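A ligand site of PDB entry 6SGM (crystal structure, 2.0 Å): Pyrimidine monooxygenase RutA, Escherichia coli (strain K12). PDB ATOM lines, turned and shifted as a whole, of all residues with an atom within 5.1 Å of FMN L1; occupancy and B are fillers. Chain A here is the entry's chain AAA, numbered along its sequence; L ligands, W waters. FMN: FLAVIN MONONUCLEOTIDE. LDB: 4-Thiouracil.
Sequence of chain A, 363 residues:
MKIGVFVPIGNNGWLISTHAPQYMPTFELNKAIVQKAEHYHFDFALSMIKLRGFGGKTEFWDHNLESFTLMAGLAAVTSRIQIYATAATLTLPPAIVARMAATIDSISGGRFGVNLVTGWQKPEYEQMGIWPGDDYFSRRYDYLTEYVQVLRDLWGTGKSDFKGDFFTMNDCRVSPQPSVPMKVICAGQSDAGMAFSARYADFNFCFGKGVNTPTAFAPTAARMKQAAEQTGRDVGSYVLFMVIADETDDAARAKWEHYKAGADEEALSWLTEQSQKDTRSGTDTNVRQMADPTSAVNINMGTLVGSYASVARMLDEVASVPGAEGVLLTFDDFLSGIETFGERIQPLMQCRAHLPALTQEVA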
ATOM      1  N   PHE A   6     -25.553   8.576  18.398  1.00  0.00           N
ATOM      2  CA  PHE A   6     -25.250   8.818  17.019  1.00  0.00           C
ATOM      3  C   PHE A   6     -26.566   8.630  16.264  1.00  0.00           C
ATOM      4  O   PHE A   6     -27.000   7.500  16.080  1.00  0.00           O
ATOM      5  CB  PHE A   6     -24.187   7.814  16.575  1.00  0.00           C
ATOM      6  CG  PHE A   6     -23.238   8.206  15.455  1.00  0.00           C
ATOM      7  CD1 PHE A   6     -23.122   9.521  15.015  1.00  0.00           C
ATOM      8  CD2 PHE A   6     -22.459   7.249  14.828  1.00  0.00           C
ATOM      9  CE1 PHE A   6     -22.257   9.862  13.972  1.00  0.00           C
ATOM     10  CE2 PHE A   6     -21.571   7.592  13.795  1.00  0.00           C
ATOM     11  CZ  PHE A   6     -21.472   8.910  13.353  1.00  0.00           C
ATOM     12  N   LEU A  46     -25.198  13.471  18.092  1.00  0.00           N
ATOM     13  CA  LEU A  46     -24.444  13.892  16.922  1.00  0.00           C
ATOM     14  C   LEU A  46     -25.036  13.224  15.678  1.00  0.00           C
ATOM     15  O   LEU A  46     -25.323  12.024  15.674  1.00  0.00           O
ATOM     16  CB  LEU A  46     -23.016  13.339  17.114  1.00  0.00           C
ATOM     17  CG  LEU A  46     -22.167  13.281  15.848  1.00  0.00           C
ATOM     18  CD1 LEU A  46     -21.745  14.711  15.412  1.00  0.00           C
ATOM     19  CD2 LEU A  46     -20.923  12.443  16.115  1.00  0.00           C
ATOM     20  N   MET A  48     -23.848  12.427  11.695  1.00  0.00           N
ATOM     21  CA  MET A  48     -22.907  12.510  10.595  1.00  0.00           C
ATOM     22  C   MET A  48     -23.527  13.244   9.417  1.00  0.00           C
ATOM     23  O   MET A  48     -24.671  13.702   9.485  1.00  0.00           O
ATOM     24  CB  MET A  48     -22.531  11.090  10.145  1.00  0.00           C
ATOM     25  CG  MET A  48     -23.749  10.248   9.730  1.00  0.00           C
ATOM     26  SD  MET A  48     -23.155   8.690   8.899  1.00  0.00           S
ATOM     27  CE  MET A  48     -24.759   8.126   8.312  1.00  0.00           C
ATOM     28  N   ILE A  49     -22.726  13.357   8.337  1.00  0.00           N
ATOM     29  CA  ILE A  49     -23.217  13.771   7.041  1.00  0.00           C
ATOM     30  C   ILE A  49     -22.785  12.677   6.061  1.00  0.00           C
ATOM     31  O   ILE A  49     -21.643  12.210   6.119  1.00  0.00           O
ATOM     32  CB  ILE A  49     -22.709  15.170   6.630  1.00  0.00           C
ATOM     33  CG1 ILE A  49     -23.329  15.687   5.309  1.00  0.00           C
ATOM     34  CG2 ILE A  49     -21.174  15.222   6.599  1.00  0.00           C
ATOM     35  CD1 ILE A  49     -24.849  15.982   5.364  1.00  0.00           C
ATOM     36  N   THR A  86     -22.368  17.816  11.715  1.00  0.00           N
ATOM     37  CA  THR A  86     -21.138  17.568  10.994  1.00  0.00           C
ATOM     38  C   THR A  86     -21.111  18.457   9.758  1.00  0.00           C
ATOM     39  O   THR A  86     -22.068  18.483   8.981  1.00  0.00           O
ATOM     40  CB  THR A  86     -21.000  16.089  10.578  1.00  0.00           C
ATOM     41  OG1 THR A  86     -21.020  15.316  11.771  1.00  0.00           O
ATOM     42  CG2 THR A  86     -19.680  15.769   9.893  1.00  0.00           C
ATOM     43  N   ASN A 115     -18.869  19.118  14.351  1.00  0.00           N
ATOM     44  CA  ASN A 115     -17.915  18.068  14.046  1.00  0.00           C
ATOM     45  C   ASN A 115     -17.360  18.374  12.663  1.00  0.00           C
ATOM     46  O   ASN A 115     -18.123  18.529  11.705  1.00  0.00           O
ATOM     47  CB  ASN A 115     -18.569  16.687  14.180  1.00  0.00           C
ATOM     48  CG  ASN A 115     -17.694  15.536  13.746  1.00  0.00           C
ATOM     49  OD1 ASN A 115     -16.497  15.515  14.005  1.00  0.00           O
ATOM     50  ND2 ASN A 115     -18.277  14.573  13.063  1.00  0.00           N
ATOM     51  N   VAL A 117     -15.102  17.397   9.487  1.00  0.00           N
ATOM     52  CA  VAL A 117     -14.536  16.276   8.770  1.00  0.00           C
ATOM     53  C   VAL A 117     -13.987  16.776   7.433  1.00  0.00           C
ATOM     54  O   VAL A 117     -14.553  17.677   6.790  1.00  0.00           O
ATOM     55  CB  VAL A 117     -15.521  15.101   8.559  1.00  0.00           C
ATOM     56  CG1 VAL A 117     -16.089  14.559   9.869  1.00  0.00           C
ATOM     57  CG2 VAL A 117     -16.633  15.479   7.602  1.00  0.00           C
ATOM     58  N   THR A 118     -12.879  16.153   7.036  1.00  0.00           N
ATOM     59  CA  THR A 118     -12.216  16.518   5.789  1.00  0.00           C
ATOM     60  C   THR A 118     -12.994  15.963   4.607  1.00  0.00           C
ATOM     61  O   THR A 118     -12.985  16.534   3.523  1.00  0.00           O
ATOM     62  CB  THR A 118     -10.784  15.968   5.797  1.00  0.00           C
ATOM     63  OG1 THR A 118     -10.897  14.556   5.991  1.00  0.00           O
ATOM     64  CG2 THR A 118      -9.925  16.564   6.912  1.00  0.00           C
ATOM     65  N   GLY A 119     -13.638  14.808   4.824  1.00  0.00           N
ATOM     66  CA  GLY A 119     -14.159  13.981   3.738  1.00  0.00           C
ATOM     67  C   GLY A 119     -13.081  12.996   3.298  1.00  0.00           C
ATOM     68  O   GLY A 119     -11.914  13.371   3.167  1.00  0.00           O
ATOM     69  N   TRP A 120     -13.477  11.737   3.085  1.00  0.00           N
ATOM     70  CA  TRP A 120     -12.529  10.728   2.622  1.00  0.00           C
ATOM     71  C   TRP A 120     -13.054  10.052   1.358  1.00  0.00           C
ATOM     72  O   TRP A 120     -12.280   9.768   0.450  1.00  0.00           O
ATOM     73  CB  TRP A 120     -12.189   9.741   3.754  1.00  0.00           C
ATOM     74  CG  TRP A 120     -12.952   8.452   3.721  1.00  0.00           C
ATOM     75  CD1 TRP A 120     -12.502   7.254   3.275  1.00  0.00           C
ATOM     76  CD2 TRP A 120     -14.317   8.237   4.157  1.00  0.00           C
ATOM     77  NE1 TRP A 120     -13.477   6.299   3.391  1.00  0.00           N
ATOM     78  CE2 TRP A 120     -14.604   6.865   3.932  1.00  0.00           C
ATOM     79  CE3 TRP A 120     -15.308   9.045   4.710  1.00  0.00           C
ATOM     80  CZ2 TRP A 120     -15.831   6.309   4.242  1.00  0.00           C
ATOM     81  CZ3 TRP A 120     -16.528   8.490   5.013  1.00  0.00           C
ATOM     82  CH2 TRP A 120     -16.786   7.141   4.778  1.00  0.00           C
ATOM     83  N   GLU A 124     -18.496  10.904  -2.952  1.00  0.00           N
ATOM     84  CA  GLU A 124     -19.439  11.826  -2.327  1.00  0.00           C
ATOM     85  C   GLU A 124     -19.262  13.242  -2.874  1.00  0.00           C
ATOM     86  O   GLU A 124     -20.228  14.013  -2.895  1.00  0.00           O
ATOM     87  CB  GLU A 124     -19.249  11.853  -0.810  1.00  0.00           C
ATOM     88  CG  GLU A 124     -19.966  10.751  -0.078  1.00  0.00           C
ATOM     89  CD  GLU A 124     -19.897  10.981   1.426  1.00  0.00           C
ATOM     90  OE1 GLU A 124     -20.520  11.966   1.901  1.00  0.00           O
ATOM     91  OE2 GLU A 124     -19.199  10.199   2.097  1.00  0.00           O
ATOM     92  N   TYR A 125     -18.031  13.557  -3.298  1.00  0.00           N
ATOM     93  CA  TYR A 125     -17.641  14.889  -3.742  1.00  0.00           C
ATOM     94  C   TYR A 125     -17.495  14.931  -5.263  1.00  0.00           C
ATOM     95  O   TYR A 125     -17.773  15.952  -5.890  1.00  0.00           O
ATOM     96  CB  TYR A 125     -16.312  15.261  -3.085  1.00  0.00           C
ATOM     97  CG  TYR A 125     -16.460  15.221  -1.594  1.00  0.00           C
ATOM     98  CD1 TYR A 125     -17.177  16.214  -0.941  1.00  0.00           C
ATOM     99  CD2 TYR A 125     -16.025  14.122  -0.864  1.00  0.00           C
ATOM    100  CE1 TYR A 125     -17.384  16.178   0.433  1.00  0.00           C
ATOM    101  CE2 TYR A 125     -16.224  14.055   0.511  1.00  0.00           C
ATOM    102  CZ  TYR A 125     -16.887  15.097   1.158  1.00  0.00           C
ATOM    103  OH  TYR A 125     -17.101  15.111   2.518  1.00  0.00           O
ATOM    104  N   ARG A 140      -5.457  17.211   3.179  1.00  0.00           N
ATOM    105  CA  ARG A 140      -6.732  17.371   3.867  1.00  0.00           C
ATOM    106  C   ARG A 140      -6.589  18.254   5.095  1.00  0.00           C
ATOM    107  O   ARG A 140      -7.400  19.151   5.315  1.00  0.00           O
ATOM    108  CB  ARG A 140      -7.193  16.027   4.423  1.00  0.00           C
ATOM    109  CG  ARG A 140      -7.537  14.995   3.365  1.00  0.00           C
ATOM    110  CD  ARG A 140      -8.143  13.791   4.002  1.00  0.00           C
ATOM    111  NE  ARG A 140      -7.263  12.859   4.687  1.00  0.00           N
ATOM    112  CZ  ARG A 140      -7.646  12.101   5.711  1.00  0.00           C
ATOM    113  NH1 ARG A 140      -8.874  12.224   6.208  1.00  0.00           N
ATOM    114  NH2 ARG A 140      -6.786  11.256   6.261  1.00  0.00           N
ATOM    115  N   TYR A 141      -5.557  17.975   5.901  1.00  0.00           N
ATOM    116  CA  TYR A 141      -5.375  18.582   7.219  1.00  0.00           C
ATOM    117  C   TYR A 141      -4.826  20.003   7.114  1.00  0.00           C
ATOM    118  O   TYR A 141      -5.104  20.839   7.987  1.00  0.00           O
ATOM    119  CB  TYR A 141      -4.731  17.580   8.196  1.00  0.00           C
ATOM    120  CG  TYR A 141      -5.748  16.573   8.695  1.00  0.00           C
ATOM    121  CD1 TYR A 141      -6.773  16.970   9.540  1.00  0.00           C
ATOM    122  CD2 TYR A 141      -5.732  15.252   8.270  1.00  0.00           C
ATOM    123  CE1 TYR A 141      -7.754  16.085   9.968  1.00  0.00           C
ATOM    124  CE2 TYR A 141      -6.698  14.351   8.696  1.00  0.00           C
ATOM    125  CZ  TYR A 141      -7.726  14.770   9.542  1.00  0.00           C
ATOM    126  OH  TYR A 141      -8.694  13.925  10.005  1.00  0.00           O
ATOM    127  N   ALA A 187     -12.791  13.794  14.160  1.00  0.00           N
ATOM    128  CA  ALA A 187     -12.734  12.351  14.248  1.00  0.00           C
ATOM    129  C   ALA A 187     -11.473  11.843  13.537  1.00  0.00           C
ATOM    130  O   ALA A 187     -11.500  10.880  12.804  1.00  0.00           O
ATOM    131  CB  ALA A 187     -14.022  11.767  13.737  1.00  0.00           C
ATOM    132  N   GLY A 188     -10.330  12.492  13.811  1.00  0.00           N
ATOM    133  CA  GLY A 188      -9.079  12.090  13.197  1.00  0.00           C
ATOM    134  C   GLY A 188      -8.534  10.808  13.831  1.00  0.00           C
ATOM    135  O   GLY A 188      -8.514  10.688  15.060  1.00  0.00           O
ATOM    136  N   GLN A 189      -8.122   9.857  12.973  1.00  0.00           N
ATOM    137  CA  GLN A 189      -7.524   8.606  13.437  1.00  0.00           C
ATOM    138  C   GLN A 189      -6.048   8.576  13.039  1.00  0.00           C
ATOM    139  O   GLN A 189      -5.229   7.984  13.725  1.00  0.00           O
ATOM    140  CB  GLN A 189      -8.176   7.348  12.843  1.00  0.00           C
ATOM    141  CG  GLN A 189      -9.691   7.272  12.919  1.00  0.00           C
ATOM    142  CD  GLN A 189     -10.226   7.365  14.327  1.00  0.00           C
ATOM    143  OE1 GLN A 189     -10.852   8.371  14.686  1.00  0.00           O
ATOM    144  NE2 GLN A 189     -10.016   6.329  15.127  1.00  0.00           N
ATOM    145  N   SER A 190      -5.731   9.171  11.887  1.00  0.00           N
ATOM    146  CA  SER A 190      -4.348   9.267  11.447  1.00  0.00           C
ATOM    147  C   SER A 190      -3.540  10.147  12.403  1.00  0.00           C
ATOM    148  O   SER A 190      -4.077  10.818  13.297  1.00  0.00           O
ATOM    149  CB  SER A 190      -4.251   9.809  10.057  1.00  0.00           C
ATOM    150  OG  SER A 190      -4.759  11.130  10.018  1.00  0.00           O
ATOM    151  N   GLY A 193      -4.466  13.613  11.751  1.00  0.00           N
ATOM    152  CA  GLY A 193      -5.809  13.877  12.214  1.00  0.00           C
ATOM    153  C   GLY A 193      -5.789  14.173  13.711  1.00  0.00           C
ATOM    154  O   GLY A 193      -6.393  15.136  14.156  1.00  0.00           O
ATOM    155  N   PHE A 205     -13.255  11.856  18.265  1.00  0.00           N
ATOM    156  CA  PHE A 205     -14.014  10.620  18.101  1.00  0.00           C
ATOM    157  C   PHE A 205     -13.110   9.551  17.510  1.00  0.00           C
ATOM    158  O   PHE A 205     -12.486   9.772  16.457  1.00  0.00           O
ATOM    159  CB  PHE A 205     -15.196  10.801  17.135  1.00  0.00           C
ATOM    160  CG  PHE A 205     -16.362  11.486  17.789  1.00  0.00           C
ATOM    161  CD1 PHE A 205     -16.951  10.965  18.937  1.00  0.00           C
ATOM    162  CD2 PHE A 205     -16.815  12.711  17.311  1.00  0.00           C
ATOM    163  CE1 PHE A 205     -17.977  11.637  19.587  1.00  0.00           C
ATOM    164  CE2 PHE A 205     -17.866  13.353  17.944  1.00  0.00           C
ATOM    165  CZ  PHE A 205     -18.431  12.831  19.087  1.00  0.00           C
ATOM    166  N   CYS A 206     -13.040   8.410  18.189  1.00  0.00           N
ATOM    167  CA  CYS A 206     -12.347   7.259  17.625  1.00  0.00           C
ATOM    168  C   CYS A 206     -13.289   6.050  17.611  1.00  0.00           C
ATOM    169  O   CYS A 206     -14.299   6.035  18.291  1.00  0.00           O
ATOM    170  CB  CYS A 206     -11.063   6.976  18.400  1.00  0.00           C
ATOM    171  SG  CYS A 206     -11.360   6.417  20.088  1.00  0.00           S
ATOM    172  N   PHE A 207     -12.913   5.045  16.822  1.00  0.00           N
ATOM    173  CA  PHE A 207     -13.683   3.817  16.663  1.00  0.00           C
ATOM    174  C   PHE A 207     -13.412   2.878  17.833  1.00  0.00           C
ATOM    175  O   PHE A 207     -12.258   2.622  18.148  1.00  0.00           O
ATOM    176  CB  PHE A 207     -13.243   3.187  15.345  1.00  0.00           C
ATOM    177  CG  PHE A 207     -13.681   3.950  14.127  1.00  0.00           C
ATOM    178  CD1 PHE A 207     -15.013   4.002  13.765  1.00  0.00           C
ATOM    179  CD2 PHE A 207     -12.761   4.642  13.353  1.00  0.00           C
ATOM    180  CE1 PHE A 207     -15.409   4.680  12.618  1.00  0.00           C
ATOM    181  CE2 PHE A 207     -13.163   5.332  12.217  1.00  0.00           C
ATOM    182  CZ  PHE A 207     -14.488   5.353  11.857  1.00  0.00           C
ATOM    183  N   LEU A 240     -16.790   5.101  19.588  1.00  0.00           N
ATOM    184  CA  LEU A 240     -18.030   4.691  18.928  1.00  0.00           C
ATOM    185  C   LEU A 240     -18.222   3.183  19.123  1.00  0.00           C
ATOM    186  O   LEU A 240     -17.329   2.390  18.775  1.00  0.00           O
ATOM    187  CB  LEU A 240     -17.912   5.007  17.445  1.00  0.00           C
ATOM    188  CG  LEU A 240     -19.053   4.497  16.564  1.00  0.00           C
ATOM    189  CD1 LEU A 240     -20.386   5.067  16.994  1.00  0.00           C
ATOM    190  CD2 LEU A 240     -18.749   4.834  15.117  1.00  0.00           C
ATOM    191  N   LEU A 328     -19.871   7.187  22.115  1.00  0.00           N
ATOM    192  CA  LEU A 328     -20.935   7.515  21.183  1.00  0.00           C
ATOM    193  C   LEU A 328     -21.623   6.190  20.801  1.00  0.00           C
ATOM    194  O   LEU A 328     -20.977   5.301  20.267  1.00  0.00           O
ATOM    195  CB  LEU A 328     -20.227   8.096  19.967  1.00  0.00           C
ATOM    196  CG  LEU A 328     -21.116   8.493  18.794  1.00  0.00           C
ATOM    197  CD1 LEU A 328     -22.089   9.601  19.207  1.00  0.00           C
ATOM    198  CD2 LEU A 328     -20.301   8.883  17.580  1.00  0.00           C
HETATM  199  N1  FMN L   1     -16.490  11.112   7.754  1.00  0.00           N
HETATM  200  C2  FMN L   1     -17.339  11.812   6.941  1.00  0.00           C
HETATM  201  O2  FMN L   1     -16.945  12.002   5.776  1.00  0.00           O
HETATM  202  N3  FMN L   1     -18.532  12.333   7.362  1.00  0.00           N
HETATM  203  C4  FMN L   1     -18.980  12.111   8.625  1.00  0.00           C
HETATM  204  O4  FMN L   1     -20.058  12.621   9.017  1.00  0.00           O
HETATM  205  C4A FMN L   1     -18.108  11.351   9.580  1.00  0.00           C
HETATM  206  N5  FMN L   1     -18.472  11.133  10.873  1.00  0.00           N
HETATM  207  C5A FMN L   1     -17.684  10.398  11.703  1.00  0.00           C
HETATM  208  C6  FMN L   1     -18.072  10.183  13.043  1.00  0.00           C
HETATM  209  C7  FMN L   1     -17.293   9.418  13.902  1.00  0.00           C
HETATM  210  C7M FMN L   1     -17.737   9.193  15.297  1.00  0.00           C
HETATM  211  C8  FMN L   1     -15.964   8.858  13.439  1.00  0.00           C
HETATM  212  C8M FMN L   1     -15.091   8.062  14.389  1.00  0.00           C
HETATM  213  C9  FMN L   1     -15.567   9.085  12.125  1.00  0.00           C
HETATM  214  C9A FMN L   1     -16.377   9.832  11.217  1.00  0.00           C
HETATM  215  N10 FMN L   1     -15.955  10.074   9.873  1.00  0.00           N
HETATM  216  C10 FMN L   1     -16.809  10.850   9.055  1.00  0.00           C
HETATM  217  C1' FMN L   1     -14.674   9.609   9.308  1.00  0.00           C
HETATM  218  C2' FMN L   1     -13.559  10.491   9.900  1.00  0.00           C
HETATM  219  O2' FMN L   1     -13.846  11.921   9.792  1.00  0.00           O
HETATM  220  C3' FMN L   1     -12.090  10.178   9.456  1.00  0.00           C
HETATM  221  O3' FMN L   1     -11.766  10.641   8.126  1.00  0.00           O
HETATM  222  C4' FMN L   1     -11.610   8.742   9.690  1.00  0.00           C
HETATM  223  O4' FMN L   1     -11.934   8.394  11.057  1.00  0.00           O
HETATM  224  C5' FMN L   1     -10.098   8.523   9.410  1.00  0.00           C
HETATM  225  O5' FMN L   1      -9.221   9.494  10.064  1.00  0.00           O
HETATM  226  P   FMN L   1      -8.241  10.519   9.270  1.00  0.00           P
HETATM  227  O1P FMN L   1      -7.579   9.679   8.228  1.00  0.00           O
HETATM  228  O2P FMN L   1      -9.156  11.627   8.728  1.00  0.00           O
HETATM  229  O3P FMN L   1      -7.341  10.966  10.398  1.00  0.00           O
HETATM  230  N01 LDB L   2     -18.258   6.179   8.885  1.00  0.00           N
HETATM  231  N02 LDB L   2     -19.669   5.579  10.808  1.00  0.00           N
HETATM  232  C01 LDB L   2     -18.509   5.312  10.025  1.00  0.00           C
HETATM  233  C02 LDB L   2     -19.110   7.257   8.519  1.00  0.00           C
HETATM  234  C03 LDB L   2     -20.273   7.421   9.423  1.00  0.00           C
HETATM  235  C04 LDB L   2     -20.527   6.641  10.474  1.00  0.00           C
HETATM  236  O01 LDB L   2     -17.736   4.379  10.309  1.00  0.00           O
HETATM  237  S01 LDB L   2     -18.811   8.168   7.263  1.00  0.00           S
HETATM  238  O   HOH W   1     -13.433  12.736   6.723  1.00  0.00           O
HETATM  239  O   HOH W   2     -11.771  14.237   9.301  1.00  0.00           O
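CZ of Phe 6 touches C6 of FMN L1, at 3.6 Å.
CB of Met 48 touches O4 of FMN L1 (3.1 Å).
Thr 86 touches FMN L1.
CG1 of Val 117 touches O2' of FMN L1, at 3.5 Å.
Gly 119 touches FMN L1 (CA to O2, 3.98 Å).
Trp 120 touches FMN L1.
Gly 188 touches FMN L1.
CA of Gly 193 touches O3P of FMN L1 (3.8 Å).
CB of Phe 205 touches C7M of FMN L1, at 3.5 Å.
CE2 of Phe 207 touches O4' of FMN L1 (3.5 Å).
CD2 of Leu 328 touches C7M of FMN L1 (3.4 Å).
Within 4 Å of FMN L1: Phe 6, Met 48, Ile 49, Thr 86, Val 117, Gly 119, Trp 120, Arg 140, Tyr 141, Ala 187, Gly 188, Gln 189, Ser 190, Gly 193, Phe 205, Phe 207 and Leu 328.
The nearest printed residue that does not touch FMN L1 is Asn 115 (4.1 Å).
Water W1 lies within hydrogen-bond range of N of Gly 119 (2.8 Å), O3' of FMN L1 (3.0 Å) and OG1 of Thr 118 (3.2 Å).
Water W2 lies within hydrogen-bond range of O2' of FMN L1, N of Thr 118 and OH of Tyr 141.
The guanidinium group (NH1) of Arg 140 lies within hydrogen-bond range of the side-chain hydroxyl (OG1) of Thr 118, at 3.1 Å.
The backbone NH of Gly 193 lies within hydrogen-bond range of the side-chain hydroxyl of Ser 190 (3.0 Å).
OE1 of Gln 189 lies close to O of Ala 187, 3.2 Å away.
The side-chain amide oxygen (OE1) of Gln 189 sits close to the backbone carbonyl oxygen (O) of Phe 205 (2.8 Å).
The side-chain hydroxyl (OG1) of Thr 86 sits at hydrogen-bond distance from the side-chain amide nitrogen (ND2) of Asn 115 (3.1 Å).
The guanidinium group (NH1) of Arg 140 lies within salt-bridge range of an oxygen (O2P) of FMN L1 (2.6 Å).
N of Ser 190 is in hydrogen-bond range of O3P of FMN L1.
The side-chain hydroxyl of Ser 190 sits at hydrogen-bond distance from an oxygen (O3P) of FMN L1, 2.6 Å away.
O2P of FMN L1 lies within hydrogen-bond range of OH of Tyr 141 (2.7 Å).
The backbone NH (N) of Ile 49 lies within hydrogen-bond range of an oxygen (O4) of FMN L1, at 2.8 Å.
O of Ile 49 is in hydrogen-bond range of N3 of FMN L1, 3.4 Å away.
An oxygen (O3P) of FMN L1 sits at hydrogen-bond distance from the backbone NH (N) of Gln 189 (2.9 Å).
The backbone carbonyl oxygen (O) of Ala 187 is in hydrogen-bond range of an oxygen (O4') of FMN L1 (3.1 Å).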
